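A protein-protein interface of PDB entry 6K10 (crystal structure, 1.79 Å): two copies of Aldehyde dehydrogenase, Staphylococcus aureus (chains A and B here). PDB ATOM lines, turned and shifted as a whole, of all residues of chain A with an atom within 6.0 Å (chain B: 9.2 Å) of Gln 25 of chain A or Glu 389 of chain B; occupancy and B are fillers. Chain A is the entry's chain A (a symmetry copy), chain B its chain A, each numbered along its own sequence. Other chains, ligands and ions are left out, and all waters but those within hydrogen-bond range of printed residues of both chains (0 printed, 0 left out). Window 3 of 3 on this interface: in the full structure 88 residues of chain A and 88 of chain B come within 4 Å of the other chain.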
ATOM      1  N   PHE A  21      16.759   8.983 -33.173  1.00  0.00           N
ATOM      2  CA  PHE A  21      17.694   9.928 -33.773  1.00  0.00           C
ATOM      3  C   PHE A  21      18.566  10.595 -32.717  1.00  0.00           C
ATOM      4  O   PHE A  21      19.761  10.814 -32.946  1.00  0.00           O
ATOM      5  CB  PHE A  21      16.961  10.990 -34.590  1.00  0.00           C
ATOM      6  CG  PHE A  21      17.889  11.946 -35.287  1.00  0.00           C
ATOM      7  CD1 PHE A  21      18.680  11.520 -36.342  1.00  0.00           C
ATOM      8  CD2 PHE A  21      17.994  13.262 -34.869  1.00  0.00           C
ATOM      9  CE1 PHE A  21      19.545  12.393 -36.978  1.00  0.00           C
ATOM     10  CE2 PHE A  21      18.857  14.139 -35.501  1.00  0.00           C
ATOM     11  CZ  PHE A  21      19.634  13.703 -36.557  1.00  0.00           C
ATOM     12  N   PHE A  22      17.990  10.939 -31.560  1.00  0.00           N
ATOM     13  CA  PHE A  22      18.814  11.488 -30.488  1.00  0.00           C
ATOM     14  C   PHE A  22      19.889  10.499 -30.065  1.00  0.00           C
ATOM     15  O   PHE A  22      21.024  10.890 -29.771  1.00  0.00           O
ATOM     16  CB  PHE A  22      17.967  11.874 -29.276  1.00  0.00           C
ATOM     17  CG  PHE A  22      18.782  12.437 -28.146  1.00  0.00           C
ATOM     18  CD1 PHE A  22      19.245  13.741 -28.194  1.00  0.00           C
ATOM     19  CD2 PHE A  22      19.136  11.646 -27.064  1.00  0.00           C
ATOM     20  CE1 PHE A  22      20.017  14.258 -27.168  1.00  0.00           C
ATOM     21  CE2 PHE A  22      19.907  12.155 -26.035  1.00  0.00           C
ATOM     22  CZ  PHE A  22      20.349  13.462 -26.088  1.00  0.00           C
ATOM     23  N   ASN A  23      19.551   9.209 -30.034  1.00  0.00           N
ATOM     24  CA  ASN A  23      20.497   8.189 -29.604  1.00  0.00           C
ATOM     25  C   ASN A  23      21.685   8.041 -30.548  1.00  0.00           C
ATOM     26  O   ASN A  23      22.674   7.406 -30.166  1.00  0.00           O
ATOM     27  CB  ASN A  23      19.780   6.847 -29.446  1.00  0.00           C
ATOM     28  CG  ASN A  23      18.875   6.814 -28.228  1.00  0.00           C
ATOM     29  OD1 ASN A  23      19.052   7.590 -27.289  1.00  0.00           O
ATOM     30  ND2 ASN A  23      17.900   5.913 -28.238  1.00  0.00           N
ATOM     31  N   THR A  24      21.623   8.609 -31.755  1.00  0.00           N
ATOM     32  CA  THR A  24      22.765   8.575 -32.662  1.00  0.00           C
ATOM     33  C   THR A  24      23.867   9.552 -32.266  1.00  0.00           C
ATOM     34  O   THR A  24      24.953   9.497 -32.855  1.00  0.00           O
ATOM     35  CB  THR A  24      22.327   8.875 -34.101  1.00  0.00           C
ATOM     36  OG1 THR A  24      21.929  10.248 -34.213  1.00  0.00           O
ATOM     37  CG2 THR A  24      21.169   7.978 -34.510  1.00  0.00           C
ATOM     38  N   GLN A  25      23.612  10.434 -31.297  1.00  0.00           N
ATOM     39  CA  GLN A  25      24.526  11.442 -30.759  1.00  0.00           C
ATOM     40  C   GLN A  25      24.761  12.607 -31.714  1.00  0.00           C
ATOM     41  O   GLN A  25      25.569  13.490 -31.399  1.00  0.00           O
ATOM     42  CB  GLN A  25      25.892  10.857 -30.364  1.00  0.00           C
ATOM     43  CG  GLN A  25      25.816   9.594 -29.518  1.00  0.00           C
ATOM     44  CD  GLN A  25      25.221   9.847 -28.150  1.00  0.00           C
ATOM     45  OE1 GLN A  25      25.750  10.639 -27.369  1.00  0.00           O
ATOM     46  NE2 GLN A  25      24.112   9.179 -27.853  1.00  0.00           N
ATOM     47  N   GLN A  26      24.074  12.656 -32.858  1.00  0.00           N
ATOM     48  CA  GLN A  26      24.371  13.679 -33.856  1.00  0.00           C
ATOM     49  C   GLN A  26      23.963  15.075 -33.394  1.00  0.00           C
ATOM     50  O   GLN A  26      24.622  16.058 -33.750  1.00  0.00           O
ATOM     51  CB  GLN A  26      23.688  13.320 -35.178  1.00  0.00           C
ATOM     52  CG  GLN A  26      23.589  14.456 -36.187  1.00  0.00           C
ATOM     53  CD  GLN A  26      24.919  14.818 -36.831  1.00  0.00           C
ATOM     54  OE1 GLN A  26      25.860  15.248 -36.159  1.00  0.00           O
ATOM     55  NE2 GLN A  26      24.997  14.659 -38.147  1.00  0.00           N
ATOM     56  N   THR A  27      22.895  15.189 -32.601  1.00  0.00           N
ATOM     57  CA  THR A  27      22.448  16.505 -32.156  1.00  0.00           C
ATOM     58  C   THR A  27      23.355  17.115 -31.094  1.00  0.00           C
ATOM     59  O   THR A  27      23.250  18.319 -30.834  1.00  0.00           O
ATOM     60  CB  THR A  27      21.014  16.436 -31.621  1.00  0.00           C
ATOM     61  OG1 THR A  27      20.993  15.729 -30.375  1.00  0.00           O
ATOM     62  CG2 THR A  27      20.108  15.729 -32.615  1.00  0.00           C
ATOM     63  N   LYS A  28      24.240  16.328 -30.480  1.00  0.00           N
ATOM     64  CA  LYS A  28      25.152  16.876 -29.484  1.00  0.00           C
ATOM     65  C   LYS A  28      26.289  17.672 -30.107  1.00  0.00           C
ATOM     66  O   LYS A  28      26.889  18.507 -29.422  1.00  0.00           O
ATOM     67  CB  LYS A  28      25.720  15.751 -28.614  1.00  0.00           C
ATOM     68  CG  LYS A  28      24.669  15.025 -27.790  1.00  0.00           C
ATOM     69  CD  LYS A  28      25.303  14.058 -26.806  1.00  0.00           C
ATOM     70  CE  LYS A  28      24.244  13.272 -26.051  1.00  0.00           C
ATOM     71  NZ  LYS A  28      24.832  12.139 -25.285  1.00  0.00           N
ATOM     72  N   ASP A  29      26.591  17.442 -31.383  1.00  0.00           N
ATOM     73  CA  ASP A  29      27.655  18.183 -32.043  1.00  0.00           C
ATOM     74  C   ASP A  29      27.261  19.645 -32.198  1.00  0.00           C
ATOM     75  O   ASP A  29      26.169  19.959 -32.683  1.00  0.00           O
ATOM     76  CB  ASP A  29      27.969  17.572 -33.407  1.00  0.00           C
ATOM     77  CG  ASP A  29      29.084  18.304 -34.128  1.00  0.00           C
ATOM     78  OD1 ASP A  29      30.266  17.981 -33.883  1.00  0.00           O
ATOM     79  OD2 ASP A  29      28.780  19.204 -34.938  1.00  0.00           O
ATOM     80  N   LYS A 435      25.742  19.423 -15.907  1.00  0.00           N
ATOM     81  CA  LYS A 435      26.318  18.201 -15.353  1.00  0.00           C
ATOM     82  C   LYS A 435      27.673  18.534 -14.742  1.00  0.00           C
ATOM     83  O   LYS A 435      28.659  18.730 -15.459  1.00  0.00           O
ATOM     84  CB  LYS A 435      26.433  17.130 -16.433  1.00  0.00           C
ATOM     85  CG  LYS A 435      26.916  15.779 -15.938  1.00  0.00           C
ATOM     86  CD  LYS A 435      26.761  14.718 -17.023  1.00  0.00           C
ATOM     87  CE  LYS A 435      27.820  14.861 -18.104  1.00  0.00           C
ATOM     88  NZ  LYS A 435      27.528  13.993 -19.283  1.00  0.00           N
ATOM     89  N   LEU B 357      34.847  -0.139 -24.765  1.00  0.00           N
ATOM     90  CA  LEU B 357      34.124   0.969 -24.142  1.00  0.00           C
ATOM     91  C   LEU B 357      32.718   1.121 -24.707  1.00  0.00           C
ATOM     92  O   LEU B 357      31.800   1.561 -23.998  1.00  0.00           O
ATOM     93  CB  LEU B 357      34.897   2.275 -24.317  1.00  0.00           C
ATOM     94  CG  LEU B 357      34.343   3.442 -23.490  1.00  0.00           C
ATOM     95  CD1 LEU B 357      34.590   3.189 -22.013  1.00  0.00           C
ATOM     96  CD2 LEU B 357      34.929   4.784 -23.922  1.00  0.00           C
ATOM     97  N   ASP B 358      32.531   0.778 -25.986  1.00  0.00           N
ATOM     98  CA  ASP B 358      31.201   0.858 -26.582  1.00  0.00           C
ATOM     99  C   ASP B 358      30.217  -0.053 -25.859  1.00  0.00           C
ATOM    100  O   ASP B 358      29.039   0.297 -25.702  1.00  0.00           O
ATOM    101  CB  ASP B 358      31.269   0.520 -28.074  1.00  0.00           C
ATOM    102  CG  ASP B 358      32.264   1.396 -28.825  1.00  0.00           C
ATOM    103  OD1 ASP B 358      31.942   2.566 -29.128  1.00  0.00           O
ATOM    104  OD2 ASP B 358      33.377   0.909 -29.117  1.00  0.00           O
ATOM    105  N   GLU B 359      30.681  -1.223 -25.410  1.00  0.00           N
ATOM    106  CA  GLU B 359      29.809  -2.121 -24.659  1.00  0.00           C
ATOM    107  C   GLU B 359      29.468  -1.543 -23.291  1.00  0.00           C
ATOM    108  O   GLU B 359      28.308  -1.593 -22.860  1.00  0.00           O
ATOM    109  CB  GLU B 359      30.468  -3.494 -24.520  1.00  0.00           C
ATOM    110  N   ALA B 360      30.457  -0.974 -22.600  1.00  0.00           N
ATOM    111  CA  ALA B 360      30.182  -0.341 -21.313  1.00  0.00           C
ATOM    112  C   ALA B 360      29.181   0.804 -21.460  1.00  0.00           C
ATOM    113  O   ALA B 360      28.236   0.923 -20.673  1.00  0.00           O
ATOM    114  CB  ALA B 360      31.486   0.155 -20.688  1.00  0.00           C
ATOM    115  N   ILE B 361      29.363   1.640 -22.483  1.00  0.00           N
ATOM    116  CA  ILE B 361      28.455   2.761 -22.727  1.00  0.00           C
ATOM    117  C   ILE B 361      27.058   2.255 -23.069  1.00  0.00           C
ATOM    118  O   ILE B 361      26.051   2.771 -22.562  1.00  0.00           O
ATOM    119  CB  ILE B 361      29.025   3.672 -23.835  1.00  0.00           C
ATOM    120  CG1 ILE B 361      30.225   4.464 -23.303  1.00  0.00           C
ATOM    121  CG2 ILE B 361      27.950   4.594 -24.408  1.00  0.00           C
ATOM    122  CD1 ILE B 361      30.924   5.314 -24.353  1.00  0.00           C
ATOM    123  N   ALA B 362      26.974   1.238 -23.932  1.00  0.00           N
ATOM    124  CA  ALA B 362      25.679   0.647 -24.261  1.00  0.00           C
ATOM    125  C   ALA B 362      24.985   0.092 -23.024  1.00  0.00           C
ATOM    126  O   ALA B 362      23.782   0.308 -22.830  1.00  0.00           O
ATOM    127  CB  ALA B 362      25.864  -0.451 -25.307  1.00  0.00           C
ATOM    128  N   ILE B 364      25.303   1.034 -19.883  1.00  0.00           N
ATOM    129  CA  ILE B 364      24.828   2.120 -19.028  1.00  0.00           C
ATOM    130  C   ILE B 364      23.659   2.850 -19.681  1.00  0.00           C
ATOM    131  O   ILE B 364      22.694   3.235 -19.005  1.00  0.00           O
ATOM    132  CB  ILE B 364      25.991   3.076 -18.690  1.00  0.00           C
ATOM    133  CG1 ILE B 364      27.071   2.337 -17.901  1.00  0.00           C
ATOM    134  CG2 ILE B 364      25.499   4.308 -17.930  1.00  0.00           C
ATOM    135  CD1 ILE B 364      28.412   3.052 -17.864  1.00  0.00           C
ATOM    136  N   HIS B 365      23.711   3.038 -21.002  1.00  0.00           N
ATOM    137  CA  HIS B 365      22.651   3.763 -21.690  1.00  0.00           C
ATOM    138  C   HIS B 365      21.343   2.979 -21.745  1.00  0.00           C
ATOM    139  O   HIS B 365      20.286   3.580 -21.961  1.00  0.00           O
ATOM    140  CB  HIS B 365      23.104   4.132 -23.106  1.00  0.00           C
ATOM    141  CG  HIS B 365      22.344   5.275 -23.705  1.00  0.00           C
ATOM    142  ND1 HIS B 365      21.076   5.135 -24.227  1.00  0.00           N
ATOM    143  CD2 HIS B 365      22.670   6.581 -23.854  1.00  0.00           C
ATOM    144  CE1 HIS B 365      20.656   6.304 -24.677  1.00  0.00           C
ATOM    145  NE2 HIS B 365      21.604   7.198 -24.462  1.00  0.00           N
ATOM    146  N   LYS B 369      19.076   7.021 -16.360  1.00  0.00           N
ATOM    147  CA  LYS B 369      20.173   7.954 -16.145  1.00  0.00           C
ATOM    148  C   LYS B 369      20.505   8.035 -14.660  1.00  0.00           C
ATOM    149  O   LYS B 369      19.639   8.420 -13.859  1.00  0.00           O
ATOM    150  CB  LYS B 369      19.814   9.333 -16.688  1.00  0.00           C
ATOM    151  CG  LYS B 369      19.485   9.339 -18.173  1.00  0.00           C
ATOM    152  CD  LYS B 369      19.054  10.716 -18.644  1.00  0.00           C
ATOM    153  CE  LYS B 369      18.862  10.747 -20.153  1.00  0.00           C
ATOM    154  NZ  LYS B 369      18.304  12.050 -20.607  1.00  0.00           N
ATOM    155  N   LEU B 373      28.086   9.176 -12.124  1.00  0.00           N
ATOM    156  CA  LEU B 373      28.874   8.251 -12.925  1.00  0.00           C
ATOM    157  C   LEU B 373      30.344   8.557 -12.694  1.00  0.00           C
ATOM    158  O   LEU B 373      30.728   9.723 -12.577  1.00  0.00           O
ATOM    159  CB  LEU B 373      28.542   8.348 -14.418  1.00  0.00           C
ATOM    160  CG  LEU B 373      29.317   7.423 -15.371  1.00  0.00           C
ATOM    161  CD1 LEU B 373      28.430   6.939 -16.507  1.00  0.00           C
ATOM    162  CD2 LEU B 373      30.557   8.115 -15.928  1.00  0.00           C
ATOM    163  N   ASN B 381      40.788  10.710 -24.453  1.00  0.00           N
ATOM    164  CA  ASN B 381      39.693  10.594 -25.406  1.00  0.00           C
ATOM    165  C   ASN B 381      38.594   9.672 -24.898  1.00  0.00           C
ATOM    166  O   ASN B 381      37.428   9.843 -25.267  1.00  0.00           O
ATOM    167  CB  ASN B 381      40.228  10.116 -26.752  1.00  0.00           C
ATOM    168  CG  ASN B 381      41.035  11.184 -27.457  1.00  0.00           C
ATOM    169  OD1 ASN B 381      41.032  12.346 -27.046  1.00  0.00           O
ATOM    170  ND2 ASN B 381      41.736  10.799 -28.514  1.00  0.00           N
ATOM    171  N   ALA B 382      38.940   8.690 -24.063  1.00  0.00           N
ATOM    172  CA  ALA B 382      37.906   7.911 -23.391  1.00  0.00           C
ATOM    173  C   ALA B 382      37.123   8.790 -22.427  1.00  0.00           C
ATOM    174  O   ALA B 382      35.892   8.709 -22.352  1.00  0.00           O
ATOM    175  CB  ALA B 382      38.529   6.725 -22.654  1.00  0.00           C
ATOM    176  N   THR B 383      37.832   9.636 -21.676  1.00  0.00           N
ATOM    177  CA  THR B 383      37.190  10.613 -20.802  1.00  0.00           C
ATOM    178  C   THR B 383      36.187  11.455 -21.574  1.00  0.00           C
ATOM    179  O   THR B 383      35.042  11.639 -21.142  1.00  0.00           O
ATOM    180  CB  THR B 383      38.256  11.501 -20.153  1.00  0.00           C
ATOM    181  OG1 THR B 383      39.238  10.681 -19.516  1.00  0.00           O
ATOM    182  CG2 THR B 383      37.642  12.442 -19.131  1.00  0.00           C
ATOM    183  N   GLN B 384      36.603  11.960 -22.735  1.00  0.00           N
ATOM    184  CA  GLN B 384      35.728  12.809 -23.533  1.00  0.00           C
ATOM    185  C   GLN B 384      34.508  12.040 -24.020  1.00  0.00           C
ATOM    186  O   GLN B 384      33.387  12.559 -23.989  1.00  0.00           O
ATOM    187  CB  GLN B 384      36.507  13.390 -24.711  1.00  0.00           C
ATOM    188  CG  GLN B 384      35.718  14.374 -25.551  1.00  0.00           C
ATOM    189  N   ARG B 385      34.704  10.795 -24.466  1.00  0.00           N
ATOM    190  CA  ARG B 385      33.584   9.987 -24.941  1.00  0.00           C
ATOM    191  C   ARG B 385      32.532   9.806 -23.855  1.00  0.00           C
ATOM    192  O   ARG B 385      31.331   9.959 -24.104  1.00  0.00           O
ATOM    193  CB  ARG B 385      34.083   8.623 -25.420  1.00  0.00           C
ATOM    194  CG  ARG B 385      34.530   8.575 -26.867  1.00  0.00           C
ATOM    195  CD  ARG B 385      34.473   7.146 -27.389  1.00  0.00           C
ATOM    196  NE  ARG B 385      33.096   6.724 -27.630  1.00  0.00           N
ATOM    197  CZ  ARG B 385      32.730   5.478 -27.914  1.00  0.00           C
ATOM    198  NH1 ARG B 385      33.640   4.517 -27.989  1.00  0.00           N
ATOM    199  NH2 ARG B 385      31.451   5.192 -28.118  1.00  0.00           N
ATOM    200  N   VAL B 386      32.966   9.481 -22.637  1.00  0.00           N
ATOM    201  CA  VAL B 386      32.022   9.171 -21.568  1.00  0.00           C
ATOM    202  C   VAL B 386      31.231  10.412 -21.172  1.00  0.00           C
ATOM    203  O   VAL B 386      30.007  10.359 -20.998  1.00  0.00           O
ATOM    204  CB  VAL B 386      32.761   8.562 -20.366  1.00  0.00           C
ATOM    205  CG1 VAL B 386      31.855   8.535 -19.158  1.00  0.00           C
ATOM    206  CG2 VAL B 386      33.239   7.159 -20.702  1.00  0.00           C
ATOM    207  N   ILE B 387      31.917  11.547 -21.020  1.00  0.00           N
ATOM    208  CA  ILE B 387      31.239  12.776 -20.612  1.00  0.00           C
ATOM    209  C   ILE B 387      30.276  13.243 -21.696  1.00  0.00           C
ATOM    210  O   ILE B 387      29.190  13.760 -21.402  1.00  0.00           O
ATOM    211  CB  ILE B 387      32.271  13.866 -20.266  1.00  0.00           C
ATOM    212  CG1 ILE B 387      33.183  13.396 -19.126  1.00  0.00           C
ATOM    213  CG2 ILE B 387      31.573  15.174 -19.915  1.00  0.00           C
ATOM    214  CD1 ILE B 387      34.375  14.296 -18.882  1.00  0.00           C
ATOM    215  N   ASN B 388      30.643  13.049 -22.964  1.00  0.00           N
ATOM    216  CA  ASN B 388      29.813  13.551 -24.052  1.00  0.00           C
ATOM    217  C   ASN B 388      28.652  12.615 -24.373  1.00  0.00           C
ATOM    218  O   ASN B 388      27.561  13.080 -24.721  1.00  0.00           O
ATOM    219  CB  ASN B 388      30.659  13.777 -25.305  1.00  0.00           C
ATOM    220  CG  ASN B 388      31.666  14.895 -25.137  1.00  0.00           C
ATOM    221  OD1 ASN B 388      31.565  15.708 -24.217  1.00  0.00           O
ATOM    222  ND2 ASN B 388      32.632  14.959 -26.044  1.00  0.00           N
ATOM    223  N   GLU B 389      28.857  11.302 -24.267  1.00  0.00           N
ATOM    224  CA  GLU B 389      27.875  10.352 -24.776  1.00  0.00           C
ATOM    225  C   GLU B 389      26.912   9.822 -23.722  1.00  0.00           C
ATOM    226  O   GLU B 389      25.831   9.347 -24.086  1.00  0.00           O
ATOM    227  CB  GLU B 389      28.581   9.167 -25.447  1.00  0.00           C
ATOM    228  CG  GLU B 389      29.372   9.558 -26.684  1.00  0.00           C
ATOM    229  CD  GLU B 389      30.123   8.391 -27.288  1.00  0.00           C
ATOM    230  OE1 GLU B 389      29.595   7.259 -27.254  1.00  0.00           O
ATOM    231  OE2 GLU B 389      31.245   8.605 -27.791  1.00  0.00           O
ATOM    232  N   LEU B 390      27.264   9.884 -22.442  1.00  0.00           N
ATOM    233  CA  LEU B 390      26.411   9.388 -21.369  1.00  0.00           C
ATOM    234  C   LEU B 390      25.922  10.551 -20.520  1.00  0.00           C
ATOM    235  O   LEU B 390      26.726  11.369 -20.060  1.00  0.00           O
ATOM    236  CB  LEU B 390      27.156   8.380 -20.493  1.00  0.00           C
ATOM    237  CG  LEU B 390      27.511   7.055 -21.167  1.00  0.00           C
ATOM    238  CD1 LEU B 390      28.404   6.225 -20.261  1.00  0.00           C
ATOM    239  CD2 LEU B 390      26.247   6.292 -21.533  1.00  0.00           C
ATOM    240  N   SER B 391      24.610  10.615 -20.312  1.00  0.00           N
ATOM    241  CA  SER B 391      24.004  11.628 -19.462  1.00  0.00           C
ATOM    242  C   SER B 391      23.777  11.069 -18.065  1.00  0.00           C
ATOM    243  O   SER B 391      23.310   9.937 -17.899  1.00  0.00           O
ATOM    244  CB  SER B 391      22.677  12.126 -20.040  1.00  0.00           C
ATOM    245  OG  SER B 391      22.078  13.067 -19.163  1.00  0.00           O
ATOM    246  N   PHE B 392      24.111  11.875 -17.066  1.00  0.00           N
ATOM    247  CA  PHE B 392      23.965  11.502 -15.669  1.00  0.00           C
ATOM    248  C   PHE B 392      23.951  12.789 -14.863  1.00  0.00           C
ATOM    249  O   PHE B 392      24.254  13.865 -15.380  1.00  0.00           O
ATOM    250  CB  PHE B 392      25.086  10.558 -15.219  1.00  0.00           C
ATOM    251  CG  PHE B 392      26.463  11.023 -15.607  1.00  0.00           C
ATOM    252  CD1 PHE B 392      27.002  10.690 -16.839  1.00  0.00           C
ATOM    253  CD2 PHE B 392      27.220  11.790 -14.737  1.00  0.00           C
ATOM    254  CE1 PHE B 392      28.267  11.115 -17.198  1.00  0.00           C
ATOM    255  CE2 PHE B 392      28.487  12.219 -15.091  1.00  0.00           C
ATOM    256  CZ  PHE B 392      29.010  11.879 -16.323  1.00  0.00           C
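O of Ile 387 of chain B is in hydrogen-bond range of NZ of Lys 435 of chain A (2.7 Å).
O of Asn 388 of chain B lies within hydrogen-bond range of NZ of Lys 28 of chain A, at 2.9 Å.
The side-chain amino group (NZ) of Lys 28 of chain A lies within hydrogen-bond range of the backbone carbonyl oxygen (O) of Glu 389 of chain B (3.2 Å).
The backbone carbonyl oxygen of Leu 390 of chain B is in hydrogen-bond range of the side-chain amino group of Lys 435 of chain A (2.9 Å).
The side-chain amide nitrogen (ND2) of Asn 388 of chain B lies close to the backbone carbonyl oxygen (O) of Gln 384 of chain B (3.2 Å).
The side-chain carboxylate of Glu 389 of chain B is in salt-bridge range of the guanidinium group of Arg 385 of chain B.
The side-chain amide nitrogen (NE2) of Gln 25 of chain A lies within hydrogen-bond range of the backbone carbonyl oxygen (O) of Asn 23 of chain A, 3.2 Å away.
The side-chain amino group (NZ) of Lys 28 of chain A sits at hydrogen-bond distance from the side-chain amide oxygen (OE1) of Gln 25 of chain A, at 2.7 Å.
Among the printed residues, merely in contact across the chains: Lys 435 of chain A with Phe 392 of chain B (3.1 Å), Asn 23 of chain A with His 365 of chain B (3.3 Å) and Gln 25 of chain A with Glu 389 of chain B (3.4 Å).
Gln 25 of chain A touches one residue of chain B.
Glu 389 of chain B touches just these residues of chain A: Gln 25 (3.4 Å) and Lys 28 (3.2 Å).
No residue of chain B comes within 4 Å of Thr 24 of chain A.
Of the printed residues of chain A, His 365 of chain B touches Asn 23 (3.3 Å).
Printed residues of chain B within 4 Å of Lys 28 of chain A: Asn 388 (2.9 Å) and Glu 389 (3.2 Å).
Of the printed residues of chain B, Asn 23 of chain A touches His 365.
Val 386 of chain B touches none of the printed residues of chain A.
Asp 29 of chain A touches none of the printed residues of chain B.
The nearest residue of chain B that does not touch Gln 25 of chain A is Asn 388 of chain B (4.03 Å).
The nearest residue of chain A that does not touch Glu 389 of chain B is Lys 435 of chain A (5.8 Å).
The nearest printed residue of chain B that does not touch Lys 435 of chain A is Ser 391 of chain B (4.2 Å).
Printed residues of chain A that touch a printed residue of chain B: Asn 23, Gln 25, Lys 28 and Lys 435.
Hydrophobic or aromatic side chains of chain B within 4 Å of the printed part of chain A: His 365 and Phe 392.
No position is printed for both chains.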
